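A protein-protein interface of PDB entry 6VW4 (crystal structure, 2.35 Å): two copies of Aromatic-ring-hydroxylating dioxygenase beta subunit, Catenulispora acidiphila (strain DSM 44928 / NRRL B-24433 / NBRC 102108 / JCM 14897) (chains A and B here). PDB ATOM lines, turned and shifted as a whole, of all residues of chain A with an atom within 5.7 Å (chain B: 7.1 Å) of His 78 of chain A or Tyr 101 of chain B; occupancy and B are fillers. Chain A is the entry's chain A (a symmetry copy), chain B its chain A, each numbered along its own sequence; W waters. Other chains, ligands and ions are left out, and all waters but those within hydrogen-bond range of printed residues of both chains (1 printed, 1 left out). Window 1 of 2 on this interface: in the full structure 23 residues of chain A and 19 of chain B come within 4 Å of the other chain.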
ATOM      1  N   MET A  22      12.422  23.197  23.377  1.00  0.00           N
ATOM      2  CA  MET A  22      12.602  24.254  22.388  1.00  0.00           C
ATOM      3  C   MET A  22      12.133  23.834  21.005  1.00  0.00           C
ATOM      4  O   MET A  22      11.755  24.695  20.207  1.00  0.00           O
ATOM      5  CB  MET A  22      14.056  24.717  22.311  1.00  0.00           C
ATOM      6  CG  MET A  22      14.585  25.413  23.519  1.00  0.00           C
ATOM      7  SD  MET A  22      13.302  26.313  24.475  1.00  0.00           S
ATOM      8  CE  MET A  22      13.535  27.836  23.427  1.00  0.00           C
ATOM      9  N   HIS A  23      12.161  22.539  20.686  1.00  0.00           N
ATOM     10  CA  HIS A  23      11.580  22.114  19.409  1.00  0.00           C
ATOM     11  C   HIS A  23      10.097  22.472  19.361  1.00  0.00           C
ATOM     12  O   HIS A  23       9.592  22.971  18.346  1.00  0.00           O
ATOM     13  CB  HIS A  23      11.773  20.609  19.161  1.00  0.00           C
ATOM     14  CG  HIS A  23      13.210  20.199  18.932  1.00  0.00           C
ATOM     15  ND1 HIS A  23      13.631  18.884  18.991  1.00  0.00           N
ATOM     16  CD2 HIS A  23      14.322  20.936  18.658  1.00  0.00           C
ATOM     17  CE1 HIS A  23      14.936  18.829  18.767  1.00  0.00           C
ATOM     18  NE2 HIS A  23      15.376  20.058  18.555  1.00  0.00           N
ATOM     19  N   LEU A  25       8.562  24.885  21.275  1.00  0.00           N
ATOM     20  CA  LEU A  25       8.408  26.338  21.264  1.00  0.00           C
ATOM     21  C   LEU A  25       8.619  26.906  19.857  1.00  0.00           C
ATOM     22  O   LEU A  25       7.791  27.683  19.347  1.00  0.00           O
ATOM     23  CB  LEU A  25       9.396  26.961  22.249  1.00  0.00           C
ATOM     24  CG  LEU A  25       9.490  28.480  22.109  1.00  0.00           C
ATOM     25  CD1 LEU A  25       8.154  29.033  22.559  1.00  0.00           C
ATOM     26  CD2 LEU A  25      10.590  29.130  22.897  1.00  0.00           C
ATOM     27  N   ASP A  26       9.723  26.511  19.206  1.00  0.00           N
ATOM     28  CA  ASP A  26      10.098  27.122  17.934  1.00  0.00           C
ATOM     29  C   ASP A  26       9.155  26.720  16.807  1.00  0.00           C
ATOM     30  O   ASP A  26       9.107  27.414  15.792  1.00  0.00           O
ATOM     31  CB  ASP A  26      11.531  26.749  17.529  1.00  0.00           C
ATOM     32  CG  ASP A  26      12.604  27.322  18.484  1.00  0.00           C
ATOM     33  OD1 ASP A  26      12.340  28.326  19.163  1.00  0.00           O
ATOM     34  OD2 ASP A  26      13.721  26.747  18.559  1.00  0.00           O
ATOM     35  N   GLU A  27       8.427  25.608  16.942  1.00  0.00           N
ATOM     36  CA  GLU A  27       7.402  25.260  15.969  1.00  0.00           C
ATOM     37  C   GLU A  27       6.028  25.791  16.367  1.00  0.00           C
ATOM     38  O   GLU A  27       5.037  25.422  15.749  1.00  0.00           O
ATOM     39  CB  GLU A  27       7.363  23.744  15.735  1.00  0.00           C
ATOM     40  CG  GLU A  27       8.695  23.123  15.186  1.00  0.00           C
ATOM     41  CD  GLU A  27       9.079  23.525  13.723  1.00  0.00           C
ATOM     42  OE1 GLU A  27      10.182  23.119  13.247  1.00  0.00           O
ATOM     43  OE2 GLU A  27       8.300  24.247  13.044  1.00  0.00           O
ATOM     44  N   ARG A  76      11.785  31.257  14.230  1.00  0.00           N
ATOM     45  CA  ARG A  76      12.779  31.431  15.270  1.00  0.00           C
ATOM     46  C   ARG A  76      13.397  30.089  15.663  1.00  0.00           C
ATOM     47  O   ARG A  76      12.779  29.032  15.521  1.00  0.00           O
ATOM     48  CB  ARG A  76      12.164  32.036  16.515  1.00  0.00           C
ATOM     49  CG  ARG A  76      11.092  33.062  16.271  1.00  0.00           C
ATOM     50  CD  ARG A  76      11.362  34.312  17.108  1.00  0.00           C
ATOM     51  NE  ARG A  76      11.555  34.015  18.525  1.00  0.00           N
ATOM     52  CZ  ARG A  76      12.077  34.867  19.401  1.00  0.00           C
ATOM     53  NH1 ARG A  76      12.459  36.071  18.998  1.00  0.00           N
ATOM     54  NH2 ARG A  76      12.225  34.514  20.672  1.00  0.00           N
ATOM     55  N   ARG A  77      14.635  30.155  16.158  1.00  0.00           N
ATOM     56  CA  ARG A  77      15.404  29.023  16.651  1.00  0.00           C
ATOM     57  C   ARG A  77      16.138  29.475  17.900  1.00  0.00           C
ATOM     58  O   ARG A  77      16.681  30.577  17.923  1.00  0.00           O
ATOM     59  CB  ARG A  77      16.448  28.520  15.657  1.00  0.00           C
ATOM     60  CG  ARG A  77      15.912  27.893  14.397  1.00  0.00           C
ATOM     61  CD  ARG A  77      15.038  26.699  14.674  1.00  0.00           C
ATOM     62  NE  ARG A  77      14.371  26.309  13.450  1.00  0.00           N
ATOM     63  CZ  ARG A  77      13.340  25.486  13.395  1.00  0.00           C
ATOM     64  NH1 ARG A  77      12.872  24.965  14.502  1.00  0.00           N
ATOM     65  NH2 ARG A  77      12.784  25.198  12.233  1.00  0.00           N
ATOM     66  N   HIS A  78      16.145  28.642  18.931  1.00  0.00           N
ATOM     67  CA  HIS A  78      16.884  28.901  20.156  1.00  0.00           C
ATOM     68  C   HIS A  78      17.975  27.861  20.266  1.00  0.00           C
ATOM     69  O   HIS A  78      17.672  26.668  20.405  1.00  0.00           O
ATOM     70  CB  HIS A  78      15.997  28.803  21.392  1.00  0.00           C
ATOM     71  CG  HIS A  78      14.979  29.875  21.464  1.00  0.00           C
ATOM     72  ND1 HIS A  78      13.836  29.857  20.705  1.00  0.00           N
ATOM     73  CD2 HIS A  78      14.939  31.015  22.191  1.00  0.00           C
ATOM     74  CE1 HIS A  78      13.138  30.952  20.949  1.00  0.00           C
ATOM     75  NE2 HIS A  78      13.776  31.660  21.862  1.00  0.00           N
ATOM     76  N   MET A  79      19.225  28.307  20.268  1.00  0.00           N
ATOM     77  CA  MET A  79      20.374  27.420  20.386  1.00  0.00           C
ATOM     78  C   MET A  79      20.983  27.517  21.764  1.00  0.00           C
ATOM     79  O   MET A  79      21.553  28.560  22.123  1.00  0.00           O
ATOM     80  CB  MET A  79      21.417  27.786  19.340  1.00  0.00           C
ATOM     81  CG  MET A  79      21.016  27.278  18.012  1.00  0.00           C
ATOM     82  SD  MET A  79      21.673  28.274  16.683  1.00  0.00           S
ATOM     83  CE  MET A  79      20.753  27.442  15.343  1.00  0.00           C
ATOM     84  N   PHE A  80      20.963  26.402  22.469  1.00  0.00           N
ATOM     85  CA  PHE A  80      21.492  26.352  23.810  1.00  0.00           C
ATOM     86  C   PHE A  80      22.923  25.845  23.754  1.00  0.00           C
ATOM     87  O   PHE A  80      23.208  24.887  23.037  1.00  0.00           O
ATOM     88  CB  PHE A  80      20.626  25.439  24.649  1.00  0.00           C
ATOM     89  CG  PHE A  80      19.278  25.996  25.020  1.00  0.00           C
ATOM     90  CD1 PHE A  80      18.786  27.143  24.441  1.00  0.00           C
ATOM     91  CD2 PHE A  80      18.474  25.321  25.958  1.00  0.00           C
ATOM     92  CE1 PHE A  80      17.545  27.641  24.812  1.00  0.00           C
ATOM     93  CE2 PHE A  80      17.241  25.813  26.323  1.00  0.00           C
ATOM     94  CZ  PHE A  80      16.770  26.968  25.746  1.00  0.00           C
ATOM     95  N   THR A 102      21.912  30.974  25.770  1.00  0.00           N
ATOM     96  CA  THR A 102      21.005  30.890  24.641  1.00  0.00           C
ATOM     97  C   THR A 102      21.427  31.897  23.590  1.00  0.00           C
ATOM     98  O   THR A 102      21.807  33.020  23.924  1.00  0.00           O
ATOM     99  CB  THR A 102      19.543  31.175  25.025  1.00  0.00           C
ATOM    100  OG1 THR A 102      19.145  30.245  26.025  1.00  0.00           O
ATOM    101  CG2 THR A 102      18.655  30.964  23.800  1.00  0.00           C
ATOM    102  N   LEU A 103      21.360  31.479  22.331  1.00  0.00           N
ATOM    103  CA  LEU A 103      21.425  32.355  21.176  1.00  0.00           C
ATOM    104  C   LEU A 103      20.131  32.260  20.368  1.00  0.00           C
ATOM    105  O   LEU A 103      19.778  31.180  19.882  1.00  0.00           O
ATOM    106  CB  LEU A 103      22.614  31.979  20.296  1.00  0.00           C
ATOM    107  CG  LEU A 103      22.826  32.931  19.108  1.00  0.00           C
ATOM    108  CD1 LEU A 103      23.166  34.314  19.580  1.00  0.00           C
ATOM    109  CD2 LEU A 103      23.912  32.423  18.164  1.00  0.00           C
ATOM    110  N   VAL A 104      19.456  33.390  20.178  1.00  0.00           N
ATOM    111  CA  VAL A 104      18.217  33.455  19.409  1.00  0.00           C
ATOM    112  C   VAL A 104      18.510  33.766  17.949  1.00  0.00           C
ATOM    113  O   VAL A 104      19.267  34.678  17.623  1.00  0.00           O
ATOM    114  CB  VAL A 104      17.269  34.505  20.012  1.00  0.00           C
ATOM    115  CG1 VAL A 104      15.922  34.467  19.315  1.00  0.00           C
ATOM    116  CG2 VAL A 104      17.130  34.268  21.500  1.00  0.00           C
ATOM    117  N   LEU A 105      17.913  32.992  17.065  1.00  0.00           N
ATOM    118  CA  LEU A 105      17.955  33.236  15.631  1.00  0.00           C
ATOM    119  C   LEU A 105      16.545  33.464  15.108  1.00  0.00           C
ATOM    120  O   LEU A 105      15.594  32.800  15.539  1.00  0.00           O
ATOM    121  CB  LEU A 105      18.575  32.088  14.903  1.00  0.00           C
ATOM    122  CG  LEU A 105      20.042  31.921  15.263  1.00  0.00           C
ATOM    123  CD1 LEU A 105      20.483  30.668  14.613  1.00  0.00           C
ATOM    124  CD2 LEU A 105      20.878  33.080  14.790  1.00  0.00           C
ATOM    125  N   MET B  79      27.634  24.144  13.231  1.00  0.00           N
ATOM    126  CA  MET B  79      27.426  24.045  14.669  1.00  0.00           C
ATOM    127  C   MET B  79      26.102  23.386  14.972  1.00  0.00           C
ATOM    128  O   MET B  79      25.039  23.965  14.699  1.00  0.00           O
ATOM    129  CB  MET B  79      27.457  25.435  15.289  1.00  0.00           C
ATOM    130  CG  MET B  79      28.850  25.915  15.407  1.00  0.00           C
ATOM    131  SD  MET B  79      28.956  27.697  15.345  1.00  0.00           S
ATOM    132  CE  MET B  79      30.778  27.782  15.282  1.00  0.00           C
ATOM    133  N   PHE B  80      26.178  22.248  15.636  1.00  0.00           N
ATOM    134  CA  PHE B  80      24.996  21.497  15.976  1.00  0.00           C
ATOM    135  C   PHE B  80      24.578  21.857  17.393  1.00  0.00           C
ATOM    136  O   PHE B  80      25.424  21.942  18.281  1.00  0.00           O
ATOM    137  CB  PHE B  80      25.297  20.020  15.861  1.00  0.00           C
ATOM    138  CG  PHE B  80      25.427  19.501  14.453  1.00  0.00           C
ATOM    139  CD1 PHE B  80      25.500  20.350  13.374  1.00  0.00           C
ATOM    140  CD2 PHE B  80      25.507  18.114  14.222  1.00  0.00           C
ATOM    141  CE1 PHE B  80      25.606  19.843  12.086  1.00  0.00           C
ATOM    142  CE2 PHE B  80      25.616  17.611  12.944  1.00  0.00           C
ATOM    143  CZ  PHE B  80      25.674  18.473  11.876  1.00  0.00           C
ATOM    144  N   THR B  81      23.267  22.047  17.614  1.00  0.00           N
ATOM    145  CA  THR B  81      22.751  22.140  18.987  1.00  0.00           C
ATOM    146  C   THR B  81      21.371  21.483  19.071  1.00  0.00           C
ATOM    147  O   THR B  81      20.780  21.115  18.053  1.00  0.00           O
ATOM    148  CB  THR B  81      22.651  23.605  19.457  1.00  0.00           C
ATOM    149  OG1 THR B  81      21.743  24.309  18.594  1.00  0.00           O
ATOM    150  CG2 THR B  81      24.006  24.298  19.475  1.00  0.00           C
ATOM    151  N   MET B  82      20.830  21.407  20.284  1.00  0.00           N
ATOM    152  CA  MET B  82      19.439  21.028  20.520  1.00  0.00           C
ATOM    153  C   MET B  82      19.154  19.614  20.065  1.00  0.00           C
ATOM    154  O   MET B  82      18.196  19.356  19.363  1.00  0.00           O
ATOM    155  CB  MET B  82      18.473  22.039  19.890  1.00  0.00           C
ATOM    156  CG  MET B  82      18.827  23.528  20.399  1.00  0.00           C
ATOM    157  SD  MET B  82      18.898  23.956  22.192  1.00  0.00           S
ATOM    158  CE  MET B  82      17.255  23.644  22.808  1.00  0.00           C
ATOM    159  N   LEU B  83      19.980  18.682  20.506  1.00  0.00           N
ATOM    160  CA  LEU B  83      19.813  17.301  20.063  1.00  0.00           C
ATOM    161  C   LEU B  83      18.743  16.611  20.908  1.00  0.00           C
ATOM    162  O   LEU B  83      18.804  16.650  22.141  1.00  0.00           O
ATOM    163  CB  LEU B  83      21.120  16.510  20.165  1.00  0.00           C
ATOM    164  CG  LEU B  83      21.056  14.974  19.939  1.00  0.00           C
ATOM    165  CD1 LEU B  83      20.745  14.733  18.467  1.00  0.00           C
ATOM    166  CD2 LEU B  83      22.389  14.314  20.295  1.00  0.00           C
ATOM    167  N   ALA B  84      17.760  15.979  20.255  1.00  0.00           N
ATOM    168  CA  ALA B  84      16.836  15.063  20.935  1.00  0.00           C
ATOM    169  C   ALA B  84      16.847  13.716  20.212  1.00  0.00           C
ATOM    170  O   ALA B  84      16.805  13.673  18.982  1.00  0.00           O
ATOM    171  CB  ALA B  84      15.414  15.643  20.991  1.00  0.00           C
ATOM    172  N   ASP B  99      16.980  14.365  16.117  1.00  0.00           N
ATOM    173  CA  ASP B  99      16.524  15.685  15.675  1.00  0.00           C
ATOM    174  C   ASP B  99      17.373  16.772  16.319  1.00  0.00           C
ATOM    175  O   ASP B  99      17.589  16.759  17.537  1.00  0.00           O
ATOM    176  CB  ASP B  99      15.057  15.933  16.037  1.00  0.00           C
ATOM    177  CG  ASP B  99      14.106  14.986  15.311  1.00  0.00           C
ATOM    178  OD1 ASP B  99      14.251  14.873  14.085  1.00  0.00           O
ATOM    179  OD2 ASP B  99      13.227  14.365  15.949  1.00  0.00           O
ATOM    180  N   PHE B 100      17.811  17.730  15.517  1.00  0.00           N
ATOM    181  CA  PHE B 100      18.677  18.759  16.040  1.00  0.00           C
ATOM    182  C   PHE B 100      18.681  19.968  15.110  1.00  0.00           C
ATOM    183  O   PHE B 100      18.088  19.960  14.037  1.00  0.00           O
ATOM    184  CB  PHE B 100      20.098  18.185  16.256  1.00  0.00           C
ATOM    185  CG  PHE B 100      20.746  17.673  15.008  1.00  0.00           C
ATOM    186  CD1 PHE B 100      20.496  16.368  14.546  1.00  0.00           C
ATOM    187  CD2 PHE B 100      21.601  18.478  14.286  1.00  0.00           C
ATOM    188  CE1 PHE B 100      21.104  15.880  13.392  1.00  0.00           C
ATOM    189  CE2 PHE B 100      22.226  17.996  13.094  1.00  0.00           C
ATOM    190  CZ  PHE B 100      21.972  16.705  12.653  1.00  0.00           C
ATOM    191  N   TYR B 101      19.360  21.018  15.573  1.00  0.00           N
ATOM    192  CA  TYR B 101      19.519  22.278  14.867  1.00  0.00           C
ATOM    193  C   TYR B 101      20.940  22.358  14.345  1.00  0.00           C
ATOM    194  O   TYR B 101      21.898  21.934  15.015  1.00  0.00           O
ATOM    195  CB  TYR B 101      19.235  23.491  15.782  1.00  0.00           C
ATOM    196  CG  TYR B 101      17.787  23.667  16.230  1.00  0.00           C
ATOM    197  CD1 TYR B 101      16.748  22.918  15.655  1.00  0.00           C
ATOM    198  CD2 TYR B 101      17.465  24.578  17.235  1.00  0.00           C
ATOM    199  CE1 TYR B 101      15.439  23.111  16.053  1.00  0.00           C
ATOM    200  CE2 TYR B 101      16.195  24.771  17.638  1.00  0.00           C
ATOM    201  CZ  TYR B 101      15.176  24.059  17.025  1.00  0.00           C
ATOM    202  OH  TYR B 101      13.897  24.265  17.460  1.00  0.00           O
ATOM    203  N   THR B 102      21.071  22.908  13.151  1.00  0.00           N
ATOM    204  CA  THR B 102      22.361  23.272  12.597  1.00  0.00           C
ATOM    205  C   THR B 102      22.382  24.765  12.331  1.00  0.00           C
ATOM    206  O   THR B 102      21.391  25.326  11.864  1.00  0.00           O
ATOM    207  CB  THR B 102      22.675  22.542  11.280  1.00  0.00           C
ATOM    208  OG1 THR B 102      22.638  21.140  11.517  1.00  0.00           O
ATOM    209  CG2 THR B 102      24.087  22.911  10.830  1.00  0.00           C
ATOM    210  N   LEU B 103      23.514  25.388  12.638  1.00  0.00           N
ATOM    211  CA  LEU B 103      23.853  26.728  12.195  1.00  0.00           C
ATOM    212  C   LEU B 103      25.115  26.696  11.333  1.00  0.00           C
ATOM    213  O   LEU B 103      26.179  26.278  11.804  1.00  0.00           O
ATOM    214  CB  LEU B 103      24.070  27.642  13.399  1.00  0.00           C
ATOM    215  CG  LEU B 103      24.320  29.110  13.019  1.00  0.00           C
ATOM    216  CD1 LEU B 103      23.120  29.704  12.343  1.00  0.00           C
ATOM    217  CD2 LEU B 103      24.700  29.951  14.234  1.00  0.00           C
ATOM    218  N   SER B 117      20.067  28.784   9.195  1.00  0.00           N
ATOM    219  CA  SER B 117      19.645  27.954  10.296  1.00  0.00           C
ATOM    220  C   SER B 117      18.846  26.792   9.720  1.00  0.00           C
ATOM    221  O   SER B 117      17.974  27.006   8.882  1.00  0.00           O
ATOM    222  CB  SER B 117      18.823  28.808  11.258  1.00  0.00           C
ATOM    223  OG  SER B 117      17.903  28.077  12.011  1.00  0.00           O
ATOM    224  N   CYS B 118      19.175  25.551  10.155  1.00  0.00           N
ATOM    225  CA  CYS B 118      18.630  24.329   9.562  1.00  0.00           C
ATOM    226  C   CYS B 118      18.215  23.265  10.576  1.00  0.00           C
ATOM    227  O   CYS B 118      19.058  22.728  11.307  1.00  0.00           O
ATOM    228  CB  CYS B 118      19.651  23.671   8.631  1.00  0.00           C
ATOM    229  SG  CYS B 118      20.332  24.648   7.288  1.00  0.00           S
ATOM    230  N   PRO B 119      16.938  22.932  10.655  1.00  0.00           N
ATOM    231  CA  PRO B 119      16.546  21.735  11.403  1.00  0.00           C
ATOM    232  C   PRO B 119      16.906  20.505  10.584  1.00  0.00           C
ATOM    233  O   PRO B 119      16.781  20.491   9.355  1.00  0.00           O
ATOM    234  CB  PRO B 119      15.026  21.884  11.585  1.00  0.00           C
ATOM    235  CG  PRO B 119      14.594  22.899  10.623  1.00  0.00           C
ATOM    236  CD  PRO B 119      15.787  23.694  10.150  1.00  0.00           C
ATOM    237  N   VAL B 120      17.414  19.488  11.268  1.00  0.00           N
ATOM    238  CA  VAL B 120      17.950  18.303  10.613  1.00  0.00           C
ATOM    239  C   VAL B 120      17.439  17.078  11.345  1.00  0.00           C
ATOM    240  O   VAL B 120      17.391  17.055  12.583  1.00  0.00           O
ATOM    241  CB  VAL B 120      19.487  18.299  10.589  1.00  0.00           C
ATOM    242  CG1 VAL B 120      20.013  17.050   9.837  1.00  0.00           C
ATOM    243  CG2 VAL B 120      20.012  19.550   9.963  1.00  0.00           C
ATOM    244  N   ASP B 142      15.680  26.852   7.029  1.00  0.00           N
ATOM    245  CA  ASP B 142      14.658  27.758   7.552  1.00  0.00           C
ATOM    246  C   ASP B 142      14.338  28.872   6.544  1.00  0.00           C
ATOM    247  O   ASP B 142      13.171  29.258   6.393  1.00  0.00           O
ATOM    248  CB  ASP B 142      15.087  28.373   8.888  1.00  0.00           C
ATOM    249  CG  ASP B 142      14.785  27.472  10.104  1.00  0.00           C
ATOM    250  OD1 ASP B 142      13.959  26.540  10.009  1.00  0.00           O
ATOM    251  OD2 ASP B 142      15.387  27.726  11.176  1.00  0.00           O
HETATM  252  O   HOH W   1      22.283  21.971  22.662  1.00  0.00           O
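Met 79 of chain A touches Leu 103 of chain B, but with the chains exchanged Leu 103 of chain A does not touch Met 79 of chain B (7.5 Å).
O of Met 82 of chain B sits at hydrogen-bond distance from NE2 of His 23 of chain A, at 3.0 Å. O of His 78 of chain A lies close to SD of Met 82 of chain B (3.5 Å). SD of Met 82 of chain B lies within hydrogen-bond range of N of Phe 80 of chain A, at 3.2 Å. The side-chain hydroxyl (OH) of Tyr 101 of chain B lies within hydrogen-bond range of the guanidinium group (NH1) of Arg 77 of chain A (3.2 Å). NH2 of Arg 77 of chain A lies within salt-bridge range of OD1 of Asp 142 of chain B. The side-chain hydroxyl (OH) of Tyr 101 of chain B is in hydrogen-bond range of the side-chain carboxylate (OD2) of Asp 26 of chain A.
Among the printed residues, pairs that only touch across the chains: Met 79 of chain A with Thr 81 of chain B (3.1 Å), Arg 77 of chain A with Ser 117 of chain B (3.1 Å), Met 22 of chain A with Met 82 of chain B (3.3 Å), Arg 77 of chain A with Pro 119 of chain B (3.3 Å), Met 22 of chain A with Tyr 101 of chain B (3.5 Å), His 23 of chain A with Tyr 101 of chain B (3.6 Å), His 23 of chain A with Asp 99 of chain B (3.6 Å), Leu 105 of chain A with Leu 103 of chain B (3.6 Å), His 78 of chain A with Tyr 101 of chain B (3.7 Å), Phe 80 of chain A with Thr 81 of chain B (3.7 Å), Met 79 of chain A with Leu 103 of chain B (3.8 Å) and His 23 of chain A with Ala 84 of chain B (3.9 Å).
His 78 of chain A touches two residues of chain B. Tyr 101 of chain B touches just these residues of chain A: Met 22, His 23, Asp 26, Arg 77 and His 78. Of the printed residues of chain A, Ala 84 of chain B touches His 23 (3.9 Å). Of the printed residues of chain A, Asp 142 of chain B touches Arg 77. Of the printed residues of chain B, Arg 77 of chain A touches Tyr 101 (3.2 Å), Ser 117 (3.1 Å), Pro 119 (3.3 Å) and Asp 142 (2.9 Å). Leu 83 of chain B touches none of the printed residues of chain A. The nearest residue of chain A that does not touch Tyr 101 of chain B is Met 79 of chain A (4.3 Å). The nearest printed residue of chain A that does not touch Met 82 of chain B is Met 79 of chain A (4.1 Å).
OG of Ser 117 of chain B lies within hydrogen-bond range of OD2 of Asp 142 of chain B (2.7 Å). A ring nitrogen (NE2) of His 78 of chain A lies within hydrogen-bond range of the guanidinium group of Arg 76 of chain A, at 3.5 Å. The backbone NH of Leu 103 of chain A sits at hydrogen-bond distance from the backbone carbonyl oxygen of Met 79 of chain A (2.9 Å). The backbone NH of Ala 84 of chain B is in hydrogen-bond range of the backbone carbonyl oxygen of Asp 99 of chain B (2.8 Å). The side-chain carboxylate (OD1) of Asp 26 of chain A is in hydrogen-bond range of a ring nitrogen (ND1) of His 78 of chain A. O of Met 79 of chain B sits at hydrogen-bond distance from N of Leu 103 of chain B.
Hydrophobic or aromatic side chains of chain A that line the printed part of chain B: Met 22, His 23, Met 79, Phe 80 and Leu 105. Printed residues of chain B that touch a printed residue of chain A: Thr 81, Met 82, Ala 84, Asp 99, Tyr 101, Leu 103, Ser 117, Pro 119 and Asp 142. Among the printed residues, 18 pairs touch across the chains. Among the printed residues, Asp or Glu carboxylates within 4 Å of a Lys or Arg side-chain nitrogen of the other chain: Arg 77 of chain A with Asp 142 of chain B (2.9 Å).
Water W1 lies within hydrogen-bond range of N of Met 82 of chain B (2.8 Å) and O of Phe 80 of chain A (3.1 Å).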
